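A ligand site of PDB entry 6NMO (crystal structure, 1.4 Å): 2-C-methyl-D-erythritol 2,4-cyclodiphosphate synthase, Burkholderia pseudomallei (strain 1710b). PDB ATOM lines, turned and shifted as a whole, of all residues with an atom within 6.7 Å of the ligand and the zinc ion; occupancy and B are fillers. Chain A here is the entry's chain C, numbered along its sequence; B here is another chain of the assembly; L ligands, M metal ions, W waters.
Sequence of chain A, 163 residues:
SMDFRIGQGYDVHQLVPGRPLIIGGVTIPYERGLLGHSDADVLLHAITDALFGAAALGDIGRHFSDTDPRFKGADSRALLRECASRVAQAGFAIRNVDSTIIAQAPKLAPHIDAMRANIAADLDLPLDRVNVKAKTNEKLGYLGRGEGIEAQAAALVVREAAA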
ATOM      1  N   TYR A  10      30.573 -22.459   0.718  1.00  0.00           N
ATOM      2  CA  TYR A  10      31.340 -21.724   1.713  1.00  0.00           C
ATOM      3  C   TYR A  10      31.422 -20.282   1.254  1.00  0.00           C
ATOM      4  O   TYR A  10      31.663 -20.003   0.083  1.00  0.00           O
ATOM      5  CB  TYR A  10      32.753 -22.339   1.792  1.00  0.00           C
ATOM      6  CG  TYR A  10      33.797 -21.463   2.434  1.00  0.00           C
ATOM      7  CD1 TYR A  10      34.631 -20.661   1.665  1.00  0.00           C
ATOM      8  CD2 TYR A  10      33.983 -21.474   3.810  1.00  0.00           C
ATOM      9  CE1 TYR A  10      35.598 -19.860   2.252  1.00  0.00           C
ATOM     10  CE2 TYR A  10      34.962 -20.683   4.403  1.00  0.00           C
ATOM     11  CZ  TYR A  10      35.765 -19.878   3.623  1.00  0.00           C
ATOM     12  OH  TYR A  10      36.722 -19.097   4.232  1.00  0.00           O
ATOM     13  N   ASP A  11      31.289 -19.349   2.197  1.00  0.00           N
ATOM     14  CA  ASP A  11      31.594 -17.959   1.871  1.00  0.00           C
ATOM     15  C   ASP A  11      32.060 -17.256   3.134  1.00  0.00           C
ATOM     16  O   ASP A  11      31.774 -17.673   4.255  1.00  0.00           O
ATOM     17  CB  ASP A  11      30.390 -17.244   1.239  1.00  0.00           C
ATOM     18  CG  ASP A  11      30.807 -16.005   0.435  1.00  0.00           C
ATOM     19  OD1 ASP A  11      32.019 -15.807   0.179  1.00  0.00           O
ATOM     20  OD2 ASP A  11      29.895 -15.221   0.071  1.00  0.00           O
ATOM     21  N   VAL A  12      32.798 -16.160   2.941  1.00  0.00           N
ATOM     22  CA  VAL A  12      33.224 -15.304   4.039  1.00  0.00           C
ATOM     23  C   VAL A  12      33.274 -13.884   3.527  1.00  0.00           C
ATOM     24  O   VAL A  12      33.714 -13.641   2.401  1.00  0.00           O
ATOM     25  CB  VAL A  12      34.572 -15.762   4.649  1.00  0.00           C
ATOM     26  CG1 VAL A  12      35.709 -15.635   3.635  1.00  0.00           C
ATOM     27  CG2 VAL A  12      34.869 -15.005   5.966  1.00  0.00           C
ATOM     28  N   HIS A  13      32.796 -12.932   4.346  1.00  0.00           N
ATOM     29  CA  HIS A  13      32.842 -11.518   4.000  1.00  0.00           C
ATOM     30  C   HIS A  13      33.474 -10.748   5.146  1.00  0.00           C
ATOM     31  O   HIS A  13      33.346 -11.122   6.317  1.00  0.00           O
ATOM     32  CB  HIS A  13      31.428 -10.925   3.772  1.00  0.00           C
ATOM     33  CG  HIS A  13      30.684 -11.491   2.603  1.00  0.00           C
ATOM     34  ND1 HIS A  13      29.326 -11.290   2.411  1.00  0.00           N
ATOM     35  CD2 HIS A  13      31.088 -12.269   1.560  1.00  0.00           C
ATOM     36  CE1 HIS A  13      28.941 -11.892   1.307  1.00  0.00           C
ATOM     37  NE2 HIS A  13      29.996 -12.494   0.758  1.00  0.00           N
ATOM     38  N   GLN A  14      34.153  -9.644   4.810  1.00  0.00           N
ATOM     39  CA  GLN A  14      34.720  -8.768   5.819  1.00  0.00           C
ATOM     40  C   GLN A  14      33.632  -7.918   6.466  1.00  0.00           C
ATOM     41  O   GLN A  14      32.639  -7.539   5.842  1.00  0.00           O
ATOM     42  CB  GLN A  14      35.749  -7.823   5.183  1.00  0.00           C
ATOM     43  CG  GLN A  14      36.985  -8.545   4.692  1.00  0.00           C
ATOM     44  CD  GLN A  14      38.073  -7.568   4.299  1.00  0.00           C
ATOM     45  OE1 GLN A  14      38.096  -7.114   3.155  1.00  0.00           O
ATOM     46  NE2 GLN A  14      38.948  -7.230   5.243  1.00  0.00           N
ATOM     47  N   LEU A  34      28.545  -6.306   6.467  1.00  0.00           N
ATOM     48  CA  LEU A  34      29.402  -7.092   5.586  1.00  0.00           C
ATOM     49  C   LEU A  34      29.667  -6.359   4.292  1.00  0.00           C
ATOM     50  O   LEU A  34      28.801  -5.667   3.745  1.00  0.00           O
ATOM     51  CB  LEU A  34      28.762  -8.437   5.319  1.00  0.00           C
ATOM     52  CG  LEU A  34      28.668  -9.302   6.578  1.00  0.00           C
ATOM     53  CD1 LEU A  34      27.865 -10.567   6.310  1.00  0.00           C
ATOM     54  CD2 LEU A  34      30.039  -9.648   7.158  1.00  0.00           C
ATOM     55  N   LEU A  35      30.903  -6.495   3.818  1.00  0.00           N
ATOM     56  CA  LEU A  35      31.388  -5.809   2.624  1.00  0.00           C
ATOM     57  C   LEU A  35      31.117  -6.680   1.400  1.00  0.00           C
ATOM     58  O   LEU A  35      31.471  -7.865   1.388  1.00  0.00           O
ATOM     59  CB  LEU A  35      32.897  -5.594   2.758  1.00  0.00           C
ATOM     60  CG  LEU A  35      33.625  -5.001   1.572  1.00  0.00           C
ATOM     61  CD1 LEU A  35      33.138  -3.564   1.314  1.00  0.00           C
ATOM     62  CD2 LEU A  35      35.117  -5.061   1.807  1.00  0.00           C
ATOM     63  N   GLY A  36      30.479  -6.108   0.391  1.00  0.00           N
ATOM     64  CA  GLY A  36      30.272  -6.836  -0.852  1.00  0.00           C
ATOM     65  C   GLY A  36      29.199  -6.203  -1.706  1.00  0.00           C
ATOM     66  O   GLY A  36      28.776  -5.063  -1.485  1.00  0.00           O
ATOM     67  N   HIS A  37      28.766  -6.970  -2.706  1.00  0.00           N
ATOM     68  CA  HIS A  37      27.713  -6.538  -3.601  1.00  0.00           C
ATOM     69  C   HIS A  37      26.394  -6.435  -2.849  1.00  0.00           C
ATOM     70  O   HIS A  37      26.022  -7.338  -2.092  1.00  0.00           O
ATOM     71  CB  HIS A  37      27.570  -7.549  -4.745  1.00  0.00           C
ATOM     72  CG  HIS A  37      26.417  -7.280  -5.660  1.00  0.00           C
ATOM     73  ND1 HIS A  37      25.327  -8.119  -5.756  1.00  0.00           N
ATOM     74  CD2 HIS A  37      26.182  -6.266  -6.527  1.00  0.00           C
ATOM     75  CE1 HIS A  37      24.473  -7.634  -6.640  1.00  0.00           C
ATOM     76  NE2 HIS A  37      24.968  -6.513  -7.120  1.00  0.00           N
ATOM     77  N   SER A  38      25.683  -5.334  -3.058  1.00  0.00           N
ATOM     78  CA  SER A  38      24.394  -5.104  -2.412  1.00  0.00           C
ATOM     79  C   SER A  38      24.510  -5.356  -0.913  1.00  0.00           C
ATOM     80  O   SER A  38      25.337  -4.739  -0.229  1.00  0.00           O
ATOM     81  CB  SER A  38      23.300  -5.970  -3.050  1.00  0.00           C
ATOM     82  OG  SER A  38      22.002  -5.528  -2.671  1.00  0.00           O
ATOM     83  N   ASP A  39      23.703  -6.289  -0.404  1.00  0.00           N
ATOM     84  CA  ASP A  39      23.641  -6.542   1.024  1.00  0.00           C
ATOM     85  C   ASP A  39      24.699  -7.537   1.530  1.00  0.00           C
ATOM     86  O   ASP A  39      24.765  -7.745   2.739  1.00  0.00           O
ATOM     87  CB  ASP A  39      22.233  -6.997   1.398  1.00  0.00           C
ATOM     88  CG  ASP A  39      21.739  -8.133   0.540  1.00  0.00           C
ATOM     89  OD1 ASP A  39      22.528  -8.678  -0.262  1.00  0.00           O
ATOM     90  OD2 ASP A  39      20.563  -8.504   0.667  1.00  0.00           O
ATOM     91  N   ALA A  40      25.501  -8.142   0.649  1.00  0.00           N
ATOM     92  CA  ALA A  40      26.652  -8.957   1.064  1.00  0.00           C
ATOM     93  C   ALA A  40      26.260 -10.033   2.066  1.00  0.00           C
ATOM     94  O   ALA A  40      26.920 -10.237   3.100  1.00  0.00           O
ATOM     95  CB  ALA A  40      27.784  -8.076   1.593  1.00  0.00           C
ATOM     96  N   ASP A  41      25.197 -10.742   1.757  1.00  0.00           N
ATOM     97  CA  ASP A  41      24.609 -11.688   2.694  1.00  0.00           C
ATOM     98  C   ASP A  41      25.354 -13.020   2.598  1.00  0.00           C
ATOM     99  O   ASP A  41      25.062 -13.868   1.742  1.00  0.00           O
ATOM    100  CB  ASP A  41      23.124 -11.836   2.400  1.00  0.00           C
ATOM    101  CG  ASP A  41      22.388 -12.606   3.464  1.00  0.00           C
ATOM    102  OD1 ASP A  41      22.966 -13.552   4.065  1.00  0.00           O
ATOM    103  OD2 ASP A  41      21.224 -12.233   3.703  1.00  0.00           O
ATOM    104  N   VAL A  42      26.326 -13.209   3.498  1.00  0.00           N
ATOM    105  CA  VAL A  42      27.254 -14.327   3.377  1.00  0.00           C
ATOM    106  C   VAL A  42      26.539 -15.663   3.490  1.00  0.00           C
ATOM    107  O   VAL A  42      26.931 -16.655   2.859  1.00  0.00           O
ATOM    108  CB  VAL A  42      28.380 -14.149   4.417  1.00  0.00           C
ATOM    109  CG1 VAL A  42      27.849 -14.256   5.863  1.00  0.00           C
ATOM    110  CG2 VAL A  42      29.530 -15.128   4.159  1.00  0.00           C
ATOM    111  N   HIS A  45      24.849 -16.399   0.164  1.00  0.00           N
ATOM    112  CA  HIS A  45      25.858 -16.764  -0.820  1.00  0.00           C
ATOM    113  C   HIS A  45      26.302 -18.220  -0.650  1.00  0.00           C
ATOM    114  O   HIS A  45      26.442 -18.957  -1.640  1.00  0.00           O
ATOM    115  CB  HIS A  45      27.063 -15.833  -0.703  1.00  0.00           C
ATOM    116  CG  HIS A  45      26.799 -14.435  -1.173  1.00  0.00           C
ATOM    117  ND1 HIS A  45      27.785 -13.473  -1.252  1.00  0.00           N
ATOM    118  CD2 HIS A  45      25.652 -13.839  -1.556  1.00  0.00           C
ATOM    119  CE1 HIS A  45      27.250 -12.341  -1.674  1.00  0.00           C
ATOM    120  NE2 HIS A  45      25.953 -12.539  -1.872  1.00  0.00           N
ATOM    121  N   ALA A  46      26.542 -18.650   0.584  1.00  0.00           N
ATOM    122  CA  ALA A  46      26.973 -20.028   0.808  1.00  0.00           C
ATOM    123  C   ALA A  46      25.898 -21.015   0.367  1.00  0.00           C
ATOM    124  O   ALA A  46      26.213 -22.049  -0.249  1.00  0.00           O
ATOM    125  CB  ALA A  46      27.337 -20.261   2.270  1.00  0.00           C
ATOM    126  N   ASP A  49      25.816 -21.181  -3.475  1.00  0.00           N
ATOM    127  CA  ASP A  49      26.881 -21.998  -4.052  1.00  0.00           C
ATOM    128  C   ASP A  49      26.628 -23.484  -3.814  1.00  0.00           C
ATOM    129  O   ASP A  49      26.932 -24.317  -4.680  1.00  0.00           O
ATOM    130  CB  ASP A  49      28.239 -21.602  -3.458  1.00  0.00           C
ATOM    131  CG  ASP A  49      29.211 -21.085  -4.479  1.00  0.00           C
ATOM    132  OD1 ASP A  49      28.825 -20.807  -5.631  1.00  0.00           O
ATOM    133  OD2 ASP A  49      30.412 -20.974  -4.115  1.00  0.00           O
ATOM    134  N   ASP A  59      29.141 -22.223 -10.210  1.00  0.00           N
ATOM    135  CA  ASP A  59      29.216 -21.449  -8.990  1.00  0.00           C
ATOM    136  C   ASP A  59      28.696 -20.038  -9.218  1.00  0.00           C
ATOM    137  O   ASP A  59      28.344 -19.648 -10.328  1.00  0.00           O
ATOM    138  CB  ASP A  59      30.644 -21.468  -8.413  1.00  0.00           C
ATOM    139  CG  ASP A  59      31.680 -20.879  -9.368  1.00  0.00           C
ATOM    140  OD1 ASP A  59      31.324 -20.162 -10.313  1.00  0.00           O
ATOM    141  OD2 ASP A  59      32.884 -21.123  -9.165  1.00  0.00           O
ATOM    142  N   ILE A  60      28.644 -19.264  -8.126  1.00  0.00           N
ATOM    143  CA  ILE A  60      28.169 -17.887  -8.205  1.00  0.00           C
ATOM    144  C   ILE A  60      28.932 -17.102  -9.269  1.00  0.00           C
ATOM    145  O   ILE A  60      28.340 -16.393 -10.085  1.00  0.00           O
ATOM    146  CB  ILE A  60      28.291 -17.214  -6.833  1.00  0.00           C
ATOM    147  CG1 ILE A  60      27.183 -17.716  -5.931  1.00  0.00           C
ATOM    148  CG2 ILE A  60      28.275 -15.685  -7.005  1.00  0.00           C
ATOM    149  CD1 ILE A  60      27.423 -17.421  -4.486  1.00  0.00           C
ATOM    150  N   GLY A  61      30.262 -17.204  -9.253  1.00  0.00           N
ATOM    151  CA  GLY A  61      31.063 -16.377 -10.128  1.00  0.00           C
ATOM    152  C   GLY A  61      30.780 -16.634 -11.585  1.00  0.00           C
ATOM    153  O   GLY A  61      30.964 -15.755 -12.428  1.00  0.00           O
ATOM    154  N   PHE A  64      26.635 -15.047 -11.995  1.00  0.00           N
ATOM    155  CA  PHE A  64      26.223 -13.684 -11.680  1.00  0.00           C
ATOM    156  C   PHE A  64      27.396 -12.766 -11.951  1.00  0.00           C
ATOM    157  O   PHE A  64      28.409 -12.816 -11.245  1.00  0.00           O
ATOM    158  CB  PHE A  64      25.695 -13.600 -10.259  1.00  0.00           C
ATOM    159  CG  PHE A  64      24.481 -14.458 -10.034  1.00  0.00           C
ATOM    160  CD1 PHE A  64      23.427 -14.418 -10.920  1.00  0.00           C
ATOM    161  CD2 PHE A  64      24.426 -15.334  -8.963  1.00  0.00           C
ATOM    162  CE1 PHE A  64      22.310 -15.211 -10.729  1.00  0.00           C
ATOM    163  CE2 PHE A  64      23.313 -16.145  -8.761  1.00  0.00           C
ATOM    164  CZ  PHE A  64      22.250 -16.091  -9.637  1.00  0.00           C
ATOM    165  N   SER A  76      20.753 -10.131  -2.324  1.00  0.00           N
ATOM    166  CA  SER A  76      21.137 -11.528  -2.213  1.00  0.00           C
ATOM    167  C   SER A  76      19.939 -12.464  -2.236  1.00  0.00           C
ATOM    168  O   SER A  76      20.059 -13.643  -2.620  1.00  0.00           O
ATOM    169  CB  SER A  76      21.943 -11.757  -0.935  1.00  0.00           C
ATOM    170  OG  SER A  76      23.137 -10.978  -0.960  1.00  0.00           O
ATOM    171  N   ALA B 134      35.128 -22.144  -7.600  1.00  0.00           N
ATOM    172  CA  ALA B 134      36.360 -21.444  -7.253  1.00  0.00           C
ATOM    173  C   ALA B 134      36.037 -20.060  -6.712  1.00  0.00           C
ATOM    174  O   ALA B 134      35.161 -19.363  -7.232  1.00  0.00           O
ATOM    175  CB  ALA B 134      37.355 -21.345  -8.427  1.00  0.00           C
ATOM    176  N   LYS B 135      36.797 -19.642  -5.706  1.00  0.00           N
ATOM    177  CA  LYS B 135      36.557 -18.324  -5.134  1.00  0.00           C
ATOM    178  C   LYS B 135      37.800 -17.846  -4.404  1.00  0.00           C
ATOM    179  O   LYS B 135      38.732 -18.622  -4.155  1.00  0.00           O
ATOM    180  CB  LYS B 135      35.385 -18.351  -4.161  1.00  0.00           C
ATOM    181  CG  LYS B 135      35.638 -19.351  -3.040  1.00  0.00           C
ATOM    182  CD  LYS B 135      34.438 -19.558  -2.120  1.00  0.00           C
ATOM    183  CE  LYS B 135      34.227 -18.367  -1.233  1.00  0.00           C
ATOM    184  NZ  LYS B 135      33.244 -17.459  -1.843  1.00  0.00           N
ATOM    185  N   THR B 136      37.791 -16.557  -4.049  1.00  0.00           N
ATOM    186  CA  THR B 136      38.804 -16.021  -3.144  1.00  0.00           C
ATOM    187  C   THR B 136      38.287 -16.122  -1.717  1.00  0.00           C
ATOM    188  O   THR B 136      37.128 -16.458  -1.468  1.00  0.00           O
ATOM    189  CB  THR B 136      39.076 -14.542  -3.434  1.00  0.00           C
ATOM    190  OG1 THR B 136      37.976 -13.754  -2.965  1.00  0.00           O
ATOM    191  CG2 THR B 136      39.308 -14.313  -4.920  1.00  0.00           C
ATOM    192  N   GLU B 138      38.143 -13.425   0.105  1.00  0.00           N
ATOM    193  CA  GLU B 138      37.769 -12.038   0.378  1.00  0.00           C
ATOM    194  C   GLU B 138      38.796 -11.356   1.275  1.00  0.00           C
ATOM    195  O   GLU B 138      38.455 -10.625   2.203  1.00  0.00           O
ATOM    196  CB  GLU B 138      36.334 -11.912   0.934  1.00  0.00           C
ATOM    197  CG  GLU B 138      35.248 -12.510   0.019  1.00  0.00           C
ATOM    198  CD  GLU B 138      35.109 -11.830  -1.343  1.00  0.00           C
ATOM    199  OE1 GLU B 138      35.510 -10.659  -1.499  1.00  0.00           O
ATOM    200  OE2 GLU B 138      34.562 -12.499  -2.269  1.00  0.00           O
HETATM  201  O1  LIG L   1      30.331  -9.404  -3.100  1.00  0.00           O
HETATM  202  S1  LIG L   1      30.359 -10.281  -1.978  1.00  0.00           S
HETATM  203  O2  LIG L   1      29.350 -10.121  -0.965  1.00  0.00           O
HETATM  204  C1  LIG L   1      31.924 -10.137  -1.208  1.00  0.00           C
HETATM  205  N1  LIG L   1      30.246 -11.815  -2.509  1.00  0.00           N
HETATM  206  C2  LIG L   1      30.985 -12.299  -3.624  1.00  0.00           C
HETATM  207  C3  LIG L   1      31.669 -11.516  -4.535  1.00  0.00           C
HETATM  208  C4  LIG L   1      30.954 -13.715  -3.802  1.00  0.00           C
HETATM  209  N2  LIG L   1      30.329 -14.461  -2.838  1.00  0.00           N
HETATM  210  C5  LIG L   1      30.301 -15.769  -3.015  1.00  0.00           C
HETATM  211  C6  LIG L   1      30.854 -16.432  -4.104  1.00  0.00           C
HETATM  212  C7  LIG L   1      31.493 -15.696  -5.062  1.00  0.00           C
HETATM  213  C8  LIG L   1      31.565 -14.288  -4.936  1.00  0.00           C
HETATM  214  C9  LIG L   1      32.247 -13.443  -5.841  1.00  0.00           C
HETATM  215  C10 LIG L   1      32.302 -12.093  -5.623  1.00  0.00           C
HETATM  216 ZN    ZN M   1      29.960 -13.504  -1.074  1.00  0.00          ZN
HETATM  217  O   HOH W   1      32.153 -13.451  -0.947  1.00  0.00           O
HETATM  218  O   HOH W   2      32.362  -7.778  -3.998  1.00  0.00           O
HETATM  219  O   HOH W   3      30.855 -18.932  -2.183  1.00  0.00           O
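O1 of the ligand sits at hydrogen-bond distance from N of His 37 (2.9 Å).
The zinc ion is bound by N2 of the ligand, OD2 of Asp 11, NE2 of His 13, ND1 of His 45, water W1 and N1 of the ligand. The zinc ion has six donor atoms within binding distance.
Water W1 lies within hydrogen-bond range of OD1 of Asp 11 (2.6 Å) and OE2 of Glu 138 of chain B (2.9 Å). Water W3 lies within hydrogen-bond range of O of Tyr 10, NZ of Lys 135 of chain B and OD2 of Asp 49.
Leu 35 touches the ligand (O to C1, 3.5 Å). Gly 36 touches the ligand. CA of Ala 40 touches O2 of the ligand, at 3.6 Å. Ile 60 touches the ligand (CD1 to C6, 3.6 Å). Lys 135 of chain B touches the ligand. Glu 138 of chain B touches the ligand. Of the 26 residues printed, 10 come within 4 Å of the ligand. The nearest printed residue that does not touch the ligand is Asp 49 (4.6 Å).
Three residues have an atom within 4 Å of the zinc ion: Asp 11, His 13 and His 45.
NZ of Lys 135 of chain B lies within salt-bridge range of OD1 of Asp 11 (2.9 Å). A ring nitrogen (ND1) of His 13 sits at hydrogen-bond distance from the backbone carbonyl oxygen (O) of Ala 40 (2.7 Å). A ring nitrogen (NE2) of His 45 lies within hydrogen-bond range of the side-chain hydroxyl (OG) of Ser 76, at 3.3 Å. The backbone carbonyl oxygen (O) of Gln 14 lies within hydrogen-bond range of the backbone NH (N) of Leu 35 (2.9 Å). OD1 of Asp 49 lies within hydrogen-bond range of N of Ile 60 (2.9 Å). OG1 of Thr 136 of chain B lies within hydrogen-bond range of N of Glu 138 of chain B, 3.1 Å away.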
